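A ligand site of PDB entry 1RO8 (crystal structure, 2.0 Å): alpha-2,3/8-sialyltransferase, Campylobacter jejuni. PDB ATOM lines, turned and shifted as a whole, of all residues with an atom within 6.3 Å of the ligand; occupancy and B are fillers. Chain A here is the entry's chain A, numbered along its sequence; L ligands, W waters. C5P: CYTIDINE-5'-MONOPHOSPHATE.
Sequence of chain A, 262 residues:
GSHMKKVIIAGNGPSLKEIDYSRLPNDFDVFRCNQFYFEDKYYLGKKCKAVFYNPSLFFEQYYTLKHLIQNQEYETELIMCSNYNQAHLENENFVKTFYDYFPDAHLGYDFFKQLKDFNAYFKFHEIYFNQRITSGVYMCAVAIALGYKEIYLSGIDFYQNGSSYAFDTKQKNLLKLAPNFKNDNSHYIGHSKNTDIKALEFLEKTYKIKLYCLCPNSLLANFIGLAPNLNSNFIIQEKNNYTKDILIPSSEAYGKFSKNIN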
ATOM      1  N   ALA A  10     -27.293  16.098 -15.366  1.00  0.00           N
ATOM      2  CA  ALA A  10     -26.839  14.939 -14.611  1.00  0.00           C
ATOM      3  C   ALA A  10     -26.916  15.102 -13.100  1.00  0.00           C
ATOM      4  O   ALA A  10     -26.313  16.007 -12.524  1.00  0.00           O
ATOM      5  CB  ALA A  10     -25.422  14.571 -15.003  1.00  0.00           C
ATOM      6  N   GLY A  11     -27.681  14.225 -12.475  1.00  0.00           N
ATOM      7  CA  GLY A  11     -27.772  14.219 -11.034  1.00  0.00           C
ATOM      8  C   GLY A  11     -26.597  13.318 -10.700  1.00  0.00           C
ATOM      9  O   GLY A  11     -25.888  12.875 -11.603  1.00  0.00           O
ATOM     10  N   ASN A  12     -26.373  13.018  -9.425  1.00  0.00           N
ATOM     11  CA  ASN A  12     -25.253  12.167  -9.048  1.00  0.00           C
ATOM     12  C   ASN A  12     -25.704  10.814  -8.501  1.00  0.00           C
ATOM     13  O   ASN A  12     -24.976  10.149  -7.769  1.00  0.00           O
ATOM     14  CB  ASN A  12     -24.388  12.898  -8.018  1.00  0.00           C
ATOM     15  CG  ASN A  12     -23.739  14.158  -8.591  1.00  0.00           C
ATOM     16  OD1 ASN A  12     -23.587  15.160  -7.907  1.00  0.00           O
ATOM     17  ND2 ASN A  12     -23.360  14.092  -9.864  1.00  0.00           N
ATOM     18  N   GLY A  13     -26.928  10.421  -8.846  1.00  0.00           N
ATOM     19  CA  GLY A  13     -27.468   9.139  -8.411  1.00  0.00           C
ATOM     20  C   GLY A  13     -26.700   7.988  -9.033  1.00  0.00           C
ATOM     21  O   GLY A  13     -25.913   8.191  -9.957  1.00  0.00           O
ATOM     22  N   PRO A  14     -26.917   6.745  -8.552  1.00  0.00           N
ATOM     23  CA  PRO A  14     -26.185   5.621  -9.136  1.00  0.00           C
ATOM     24  C   PRO A  14     -26.433   5.376 -10.628  1.00  0.00           C
ATOM     25  O   PRO A  14     -25.620   4.754 -11.291  1.00  0.00           O
ATOM     26  CB  PRO A  14     -26.594   4.441  -8.247  1.00  0.00           C
ATOM     27  CG  PRO A  14     -27.944   4.809  -7.783  1.00  0.00           C
ATOM     28  CD  PRO A  14     -27.824   6.286  -7.483  1.00  0.00           C
ATOM     29  N   CYS A  33     -23.661  18.964 -11.040  1.00  0.00           N
ATOM     30  CA  CYS A  33     -23.919  19.596  -9.743  1.00  0.00           C
ATOM     31  C   CYS A  33     -23.179  18.955  -8.553  1.00  0.00           C
ATOM     32  O   CYS A  33     -22.716  17.817  -8.618  1.00  0.00           O
ATOM     33  CB  CYS A  33     -25.422  19.618  -9.445  1.00  0.00           C
ATOM     34  SG  CYS A  33     -26.120  18.030  -8.907  1.00  0.00           S
ATOM     35  N   ASN A  34     -23.064  19.732  -7.486  1.00  0.00           N
ATOM     36  CA  ASN A  34     -22.449  19.316  -6.232  1.00  0.00           C
ATOM     37  C   ASN A  34     -21.160  18.489  -6.320  1.00  0.00           C
ATOM     38  O   ASN A  34     -20.125  18.979  -6.751  1.00  0.00           O
ATOM     39  CB  ASN A  34     -23.507  18.583  -5.402  1.00  0.00           C
ATOM     40  CG  ASN A  34     -24.739  19.455  -5.123  1.00  0.00           C
ATOM     41  OD1 ASN A  34     -25.790  18.967  -4.700  1.00  0.00           O
ATOM     42  ND2 ASN A  34     -24.592  20.753  -5.346  1.00  0.00           N
ATOM     43  N   GLN A  35     -21.209  17.217  -5.903  1.00  0.00           N
ATOM     44  CA  GLN A  35     -20.004  16.382  -5.920  1.00  0.00           C
ATOM     45  C   GLN A  35     -19.749  15.570  -7.199  1.00  0.00           C
ATOM     46  O   GLN A  35     -19.211  14.469  -7.147  1.00  0.00           O
ATOM     47  CB  GLN A  35     -20.014  15.418  -4.719  1.00  0.00           C
ATOM     48  CG  GLN A  35     -19.774  16.086  -3.356  1.00  0.00           C
ATOM     49  CD  GLN A  35     -20.891  17.025  -2.941  1.00  0.00           C
ATOM     50  OE1 GLN A  35     -20.751  18.243  -3.010  1.00  0.00           O
ATOM     51  NE2 GLN A  35     -22.019  16.459  -2.518  1.00  0.00           N
ATOM     52  N   ASN A  54     -25.077  24.213  -4.066  1.00  0.00           N
ATOM     53  CA  ASN A  54     -25.988  24.739  -3.057  1.00  0.00           C
ATOM     54  C   ASN A  54     -25.292  25.892  -2.340  1.00  0.00           C
ATOM     55  O   ASN A  54     -24.074  25.903  -2.214  1.00  0.00           O
ATOM     56  CB  ASN A  54     -26.368  23.650  -2.050  1.00  0.00           C
ATOM     57  CG  ASN A  54     -27.201  22.551  -2.693  1.00  0.00           C
ATOM     58  OD1 ASN A  54     -28.240  22.814  -3.294  1.00  0.00           O
ATOM     59  ND2 ASN A  54     -26.739  21.310  -2.548  1.00  0.00           N
ATOM     60  N   THR A 134     -35.351  18.473  -5.936  1.00  0.00           N
ATOM     61  CA  THR A 134     -33.912  18.258  -5.804  1.00  0.00           C
ATOM     62  C   THR A 134     -33.133  19.113  -6.809  1.00  0.00           C
ATOM     63  O   THR A 134     -33.732  19.780  -7.647  1.00  0.00           O
ATOM     64  CB  THR A 134     -33.551  16.775  -6.032  1.00  0.00           C
ATOM     65  OG1 THR A 134     -33.972  16.380  -7.339  1.00  0.00           O
ATOM     66  CG2 THR A 134     -34.251  15.890  -5.010  1.00  0.00           C
ATOM     67  N   SER A 135     -31.803  19.070  -6.733  1.00  0.00           N
ATOM     68  CA  SER A 135     -30.947  19.837  -7.646  1.00  0.00           C
ATOM     69  C   SER A 135     -31.181  19.437  -9.108  1.00  0.00           C
ATOM     70  O   SER A 135     -31.068  20.272 -10.003  1.00  0.00           O
ATOM     71  CB  SER A 135     -29.472  19.630  -7.294  1.00  0.00           C
ATOM     72  OG  SER A 135     -29.080  20.422  -6.198  1.00  0.00           O
ATOM     73  N   GLY A 136     -31.477  18.167  -9.331  1.00  0.00           N
ATOM     74  CA  GLY A 136     -31.723  17.690 -10.679  1.00  0.00           C
ATOM     75  C   GLY A 136     -32.851  18.455 -11.350  1.00  0.00           C
ATOM     76  O   GLY A 136     -32.750  18.807 -12.516  1.00  0.00           O
ATOM     77  N   VAL A 137     -33.915  18.709 -10.600  1.00  0.00           N
ATOM     78  CA  VAL A 137     -35.064  19.424 -11.132  1.00  0.00           C
ATOM     79  C   VAL A 137     -34.774  20.911 -11.237  1.00  0.00           C
ATOM     80  O   VAL A 137     -35.164  21.562 -12.215  1.00  0.00           O
ATOM     81  CB  VAL A 137     -36.295  19.185 -10.250  1.00  0.00           C
ATOM     82  CG1 VAL A 137     -37.512  19.917 -10.822  1.00  0.00           C
ATOM     83  CG2 VAL A 137     -36.574  17.685 -10.168  1.00  0.00           C
ATOM     84  N   MET A 139     -32.014  22.305 -11.920  1.00  0.00           N
ATOM     85  CA  MET A 139     -31.234  22.479 -13.151  1.00  0.00           C
ATOM     86  C   MET A 139     -32.115  22.453 -14.406  1.00  0.00           C
ATOM     87  O   MET A 139     -31.836  23.154 -15.379  1.00  0.00           O
ATOM     88  CB  MET A 139     -30.154  21.404 -13.233  1.00  0.00           C
ATOM     89  CG  MET A 139     -29.041  21.586 -12.200  1.00  0.00           C
ATOM     90  SD  MET A 139     -27.548  20.380 -12.440  1.00  0.00           S
ATOM     91  CE  MET A 139     -28.383  18.786 -11.744  1.00  0.00           C
ATOM     92  N   GLY A 155     -28.666  10.219 -13.825  1.00  0.00           N
ATOM     93  CA  GLY A 155     -28.288  10.358 -12.433  1.00  0.00           C
ATOM     94  C   GLY A 155     -29.374  10.841 -11.479  1.00  0.00           C
ATOM     95  O   GLY A 155     -29.068  11.365 -10.407  1.00  0.00           O
ATOM     96  N   ILE A 156     -30.630  10.685 -11.873  1.00  0.00           N
ATOM     97  CA  ILE A 156     -31.748  11.082 -11.017  1.00  0.00           C
ATOM     98  C   ILE A 156     -32.468   9.794 -10.642  1.00  0.00           C
ATOM     99  O   ILE A 156     -33.171   9.201 -11.441  1.00  0.00           O
ATOM    100  CB  ILE A 156     -32.707  12.047 -11.755  1.00  0.00           C
ATOM    101  CG1 ILE A 156     -31.982  13.378 -12.004  1.00  0.00           C
ATOM    102  CG2 ILE A 156     -33.977  12.282 -10.931  1.00  0.00           C
ATOM    103  CD1 ILE A 156     -32.838  14.439 -12.661  1.00  0.00           C
ATOM    104  N   ASP A 157     -32.257   9.357  -9.402  1.00  0.00           N
ATOM    105  CA  ASP A 157     -32.826   8.108  -8.929  1.00  0.00           C
ATOM    106  C   ASP A 157     -33.785   8.219  -7.743  1.00  0.00           C
ATOM    107  O   ASP A 157     -34.342   7.217  -7.311  1.00  0.00           O
ATOM    108  CB  ASP A 157     -31.690   7.145  -8.588  1.00  0.00           C
ATOM    109  CG  ASP A 157     -30.899   6.739  -9.811  1.00  0.00           C
ATOM    110  OD1 ASP A 157     -29.685   7.043  -9.871  1.00  0.00           O
ATOM    111  OD2 ASP A 157     -31.496   6.113 -10.709  1.00  0.00           O
ATOM    112  N   PHE A 158     -33.948   9.431  -7.227  1.00  0.00           N
ATOM    113  CA  PHE A 158     -34.840   9.693  -6.101  1.00  0.00           C
ATOM    114  C   PHE A 158     -34.419   8.996  -4.808  1.00  0.00           C
ATOM    115  O   PHE A 158     -35.265   8.584  -4.004  1.00  0.00           O
ATOM    116  CB  PHE A 158     -36.270   9.279  -6.485  1.00  0.00           C
ATOM    117  CG  PHE A 158     -36.710   9.797  -7.829  1.00  0.00           C
ATOM    118  CD1 PHE A 158     -36.981   8.911  -8.880  1.00  0.00           C
ATOM    119  CD2 PHE A 158     -36.817  11.161  -8.063  1.00  0.00           C
ATOM    120  CE1 PHE A 158     -37.362   9.392 -10.134  1.00  0.00           C
ATOM    121  CE2 PHE A 158     -37.198  11.643  -9.317  1.00  0.00           C
ATOM    122  CZ  PHE A 158     -37.475  10.749 -10.358  1.00  0.00           C
ATOM    123  N   TYR A 159     -33.108   8.870  -4.608  1.00  0.00           N
ATOM    124  CA  TYR A 159     -32.538   8.244  -3.416  1.00  0.00           C
ATOM    125  C   TYR A 159     -33.167   6.895  -3.079  1.00  0.00           C
ATOM    126  O   TYR A 159     -33.929   6.772  -2.118  1.00  0.00           O
ATOM    127  CB  TYR A 159     -32.666   9.198  -2.226  1.00  0.00           C
ATOM    128  CG  TYR A 159     -32.017  10.541  -2.464  1.00  0.00           C
ATOM    129  CD1 TYR A 159     -32.692  11.561  -3.138  1.00  0.00           C
ATOM    130  CD2 TYR A 159     -30.694  10.773  -2.090  1.00  0.00           C
ATOM    131  CE1 TYR A 159     -32.073  12.784  -3.428  1.00  0.00           C
ATOM    132  CE2 TYR A 159     -30.053  11.986  -2.373  1.00  0.00           C
ATOM    133  CZ  TYR A 159     -30.759  12.979  -3.047  1.00  0.00           C
ATOM    134  OH  TYR A 159     -30.133  14.180  -3.330  1.00  0.00           O
ATOM    135  N   GLN A 160     -32.818   5.875  -3.857  1.00  0.00           N
ATOM    136  CA  GLN A 160     -33.339   4.521  -3.677  1.00  0.00           C
ATOM    137  C   GLN A 160     -32.724   3.719  -2.542  1.00  0.00           C
ATOM    138  O   GLN A 160     -33.086   2.563  -2.347  1.00  0.00           O
ATOM    139  CB  GLN A 160     -33.187   3.735  -4.991  1.00  0.00           C
ATOM    140  CG  GLN A 160     -34.111   4.208  -6.078  1.00  0.00           C
ATOM    141  CD  GLN A 160     -35.567   4.038  -5.697  1.00  0.00           C
ATOM    142  OE1 GLN A 160     -36.062   2.912  -5.604  1.00  0.00           O
ATOM    143  NE2 GLN A 160     -36.253   5.148  -5.466  1.00  0.00           N
ATOM    144  N   ASN A 161     -31.806   4.321  -1.798  1.00  0.00           N
ATOM    145  CA  ASN A 161     -31.156   3.631  -0.674  1.00  0.00           C
ATOM    146  C   ASN A 161     -30.182   2.550  -1.120  1.00  0.00           C
ATOM    147  O   ASN A 161     -29.018   2.538  -0.685  1.00  0.00           O
ATOM    148  CB  ASN A 161     -32.216   3.010   0.241  1.00  0.00           C
ATOM    149  CG  ASN A 161     -33.100   4.052   0.905  1.00  0.00           C
ATOM    150  OD1 ASN A 161     -33.648   4.938   0.239  1.00  0.00           O
ATOM    151  ND2 ASN A 161     -33.248   3.957   2.231  1.00  0.00           N
ATOM    152  N   SER A 163     -28.297   2.248  -3.327  1.00  0.00           N
ATOM    153  CA  SER A 163     -27.037   2.925  -3.620  1.00  0.00           C
ATOM    154  C   SER A 163     -27.376   4.410  -3.557  1.00  0.00           C
ATOM    155  O   SER A 163     -28.284   4.872  -4.242  1.00  0.00           O
ATOM    156  CB  SER A 163     -26.522   2.545  -4.999  1.00  0.00           C
ATOM    157  OG  SER A 163     -25.219   3.080  -5.214  1.00  0.00           O
ATOM    158  N   SER A 164     -26.652   5.148  -2.732  1.00  0.00           N
ATOM    159  CA  SER A 164     -26.920   6.568  -2.585  1.00  0.00           C
ATOM    160  C   SER A 164     -26.388   7.431  -3.730  1.00  0.00           C
ATOM    161  O   SER A 164     -27.081   8.322  -4.205  1.00  0.00           O
ATOM    162  CB  SER A 164     -26.347   7.061  -1.254  1.00  0.00           C
ATOM    163  OG  SER A 164     -27.045   8.205  -0.804  1.00  0.00           O
ATOM    164  N   TYR A 165     -25.164   7.164  -4.177  1.00  0.00           N
ATOM    165  CA  TYR A 165     -24.569   7.925  -5.282  1.00  0.00           C
ATOM    166  C   TYR A 165     -23.798   7.010  -6.221  1.00  0.00           C
ATOM    167  O   TYR A 165     -23.630   5.821  -5.942  1.00  0.00           O
ATOM    168  CB  TYR A 165     -23.638   9.015  -4.754  1.00  0.00           C
ATOM    169  CG  TYR A 165     -24.319  10.069  -3.910  1.00  0.00           C
ATOM    170  CD1 TYR A 165     -24.374   9.960  -2.527  1.00  0.00           C
ATOM    171  CD2 TYR A 165     -24.952  11.163  -4.520  1.00  0.00           C
ATOM    172  CE1 TYR A 165     -25.029  10.921  -1.759  1.00  0.00           C
ATOM    173  CE2 TYR A 165     -25.608  12.125  -3.762  1.00  0.00           C
ATOM    174  CZ  TYR A 165     -25.650  12.001  -2.382  1.00  0.00           C
ATOM    175  OH  TYR A 165     -26.300  12.956  -1.626  1.00  0.00           O
ATOM    176  N   HIS A 191     -37.285  15.547   0.393  1.00  0.00           N
ATOM    177  CA  HIS A 191     -37.423  15.266  -1.056  1.00  0.00           C
ATOM    178  C   HIS A 191     -38.055  13.895  -1.280  1.00  0.00           C
ATOM    179  O   HIS A 191     -38.028  13.036  -0.395  1.00  0.00           O
ATOM    180  CB  HIS A 191     -36.051  15.299  -1.737  1.00  0.00           C
ATOM    181  CG  HIS A 191     -35.307  16.584  -1.537  1.00  0.00           C
ATOM    182  ND1 HIS A 191     -34.718  16.934  -0.338  1.00  0.00           N
ATOM    183  CD2 HIS A 191     -35.054  17.610  -2.395  1.00  0.00           C
ATOM    184  CE1 HIS A 191     -34.138  18.114  -0.465  1.00  0.00           C
ATOM    185  NE2 HIS A 191     -34.333  18.549  -1.697  1.00  0.00           N
ATOM    186  N   ASP A 196     -40.459  15.355  -7.261  1.00  0.00           N
ATOM    187  CA  ASP A 196     -39.635  15.633  -8.434  1.00  0.00           C
ATOM    188  C   ASP A 196     -40.377  15.337  -9.740  1.00  0.00           C
ATOM    189  O   ASP A 196     -40.362  16.147 -10.656  1.00  0.00           O
ATOM    190  CB  ASP A 196     -38.343  14.820  -8.398  1.00  0.00           C
ATOM    191  CG  ASP A 196     -37.260  15.477  -7.566  1.00  0.00           C
ATOM    192  OD1 ASP A 196     -36.148  14.891  -7.450  1.00  0.00           O
ATOM    193  OD2 ASP A 196     -37.504  16.570  -7.015  1.00  0.00           O
HETATM  194  O3P C5P L   1     -27.531  14.432  -3.465  1.00  0.00           O
HETATM  195  P   C5P L   1     -27.105  15.766  -4.143  1.00  0.00           P
HETATM  196  O1P C5P L   1     -28.180  16.880  -4.097  1.00  0.00           O
HETATM  197  O2P C5P L   1     -25.806  16.274  -3.549  1.00  0.00           O
HETATM  198  O5' C5P L   1     -26.711  15.772  -5.561  1.00  0.00           O
HETATM  199  C5' C5P L   1     -27.505  14.885  -6.345  1.00  0.00           C
HETATM  200  C4' C5P L   1     -28.702  15.175  -7.127  1.00  0.00           C
HETATM  201  O4' C5P L   1     -28.903  13.954  -7.792  1.00  0.00           O
HETATM  202  C3' C5P L   1     -29.964  15.463  -6.328  1.00  0.00           C
HETATM  203  O3' C5P L   1     -30.154  16.883  -6.241  1.00  0.00           O
HETATM  204  C2' C5P L   1     -31.000  14.779  -7.210  1.00  0.00           C
HETATM  205  O2' C5P L   1     -31.471  15.491  -8.353  1.00  0.00           O
HETATM  206  C1' C5P L   1     -30.249  13.530  -7.528  1.00  0.00           C
HETATM  207  N1  C5P L   1     -30.014  12.162  -6.974  1.00  0.00           N
HETATM  208  C2  C5P L   1     -31.060  11.151  -7.104  1.00  0.00           C
HETATM  209  N3  C5P L   1     -30.925   9.916  -6.512  1.00  0.00           N
HETATM  210  C4  C5P L   1     -29.826   9.572  -5.684  1.00  0.00           C
HETATM  211  C5  C5P L   1     -28.839  10.515  -5.475  1.00  0.00           C
HETATM  212  C6  C5P L   1     -28.810  11.681  -6.146  1.00  0.00           C
HETATM  213  O2  C5P L   1     -32.161  11.408  -7.790  1.00  0.00           O
HETATM  214  N4  C5P L   1     -29.744   8.352  -5.124  1.00  0.00           N
HETATM  215  O   HOH W   1     -34.232  12.839  -6.842  1.00  0.00           O
HETATM  216  O   HOH W   2     -23.557  15.285  -5.124  1.00  0.00           O
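O2 of the ligand is in hydrogen-bond range of N of Asp 157.
The backbone NH (N) of Tyr 159 is in hydrogen-bond range of a nitrogen (N3) of the ligand, 3.1 Å away.
The side-chain hydroxyl (OH) of Tyr 159 is in hydrogen-bond range of an oxygen (O3P) of the ligand.
The side-chain hydroxyl (OH) of Tyr 165 is in hydrogen-bond range of an oxygen (O3P) of the ligand.
The backbone NH (N) of Phe 158 is in hydrogen-bond range of an oxygen (O2) of the ligand, at 2.7 Å.
An oxygen (O3') of the ligand sits at hydrogen-bond distance from the backbone NH (N) of Ser 135 (2.8 Å).
O of Ser 164 is in hydrogen-bond range of N4 of the ligand (2.8 Å).
The side-chain hydroxyl of Thr 134 lies within hydrogen-bond range of an oxygen (O2') of the ligand, 2.8 Å away.
The backbone NH of Gly 136 sits at hydrogen-bond distance from an oxygen (O2') of the ligand, at 2.8 Å.
The side-chain amide oxygen (OD1) of Asn 34 lies close to an oxygen (O2P) of the ligand.
An oxygen (O4') of the ligand sits at hydrogen-bond distance from the backbone NH of Asn 12 (3.2 Å).
The backbone carbonyl oxygen (O) of Asp 157 lies close to the side-chain amide nitrogen (NE2) of Gln 160, at 3.4 Å.
The side-chain amide oxygen of Asn 161 lies close to the backbone carbonyl oxygen of Tyr 159 (3.0 Å).
The backbone carbonyl oxygen of Tyr 165 is in hydrogen-bond range of the side-chain hydroxyl of Ser 163.
The side-chain hydroxyl (OG1) of Thr 134 is in hydrogen-bond range of the side-chain carboxylate (OD1) of Asp 196 (2.6 Å).
OD1 of Asn 34 is in hydrogen-bond range of ND2 of Asn 54 (3.3 Å).
N of Asn 12 is in hydrogen-bond range of O of Gly 155 (3.3 Å).
The backbone carbonyl oxygen (O) of Cys 33 sits close to the side-chain amide oxygen (OD1) of Asn 12 (2.9 Å).
The backbone carbonyl oxygen (O) of Gly 155 lies within hydrogen-bond range of the backbone NH (N) of Gly 13 (2.8 Å).
CA of Gly 11 touches O4' of the ligand, at 3.4 Å.
Gly 13 touches the ligand.
CD of Pro 14 touches N4 of the ligand, at 3.7 Å.
Gln 35 touches the ligand (NE2 to O2P, 3.9 Å).
Gly 155 touches the ligand.
Ile 156 touches the ligand.
O of Ser 163 touches N4 of the ligand, at 3.9 Å.
Hydrophobic or aromatic side chains within 4 Å of the ligand: Pro 14, Ile 156, Tyr 159 and Tyr 165.
17 residues have an atom within 4 Å of the ligand: Gly 11, Asn 12, Gly 13, Pro 14, Asn 34, Gln 35, Thr 134, Ser 135, Gly 136, Gly 155, Ile 156, Asp 157, Phe 158, Tyr 159, Ser 163, Ser 164 and Tyr 165.
The nearest printed residue that does not touch the ligand is Cys 33 (4.1 Å).
Water W1 lies within hydrogen-bond range of O2 of the ligand (2.7 Å), OD1 of Asp 196 (2.9 Å) and N of Phe 158 (3.4 Å).
Water W2 lies within hydrogen-bond range of the side-chain amide oxygen of Asn 12 (2.8 Å), an oxygen (O2P) of the ligand (2.9 Å) and the backbone NH of Gln 35 (3.1 Å).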
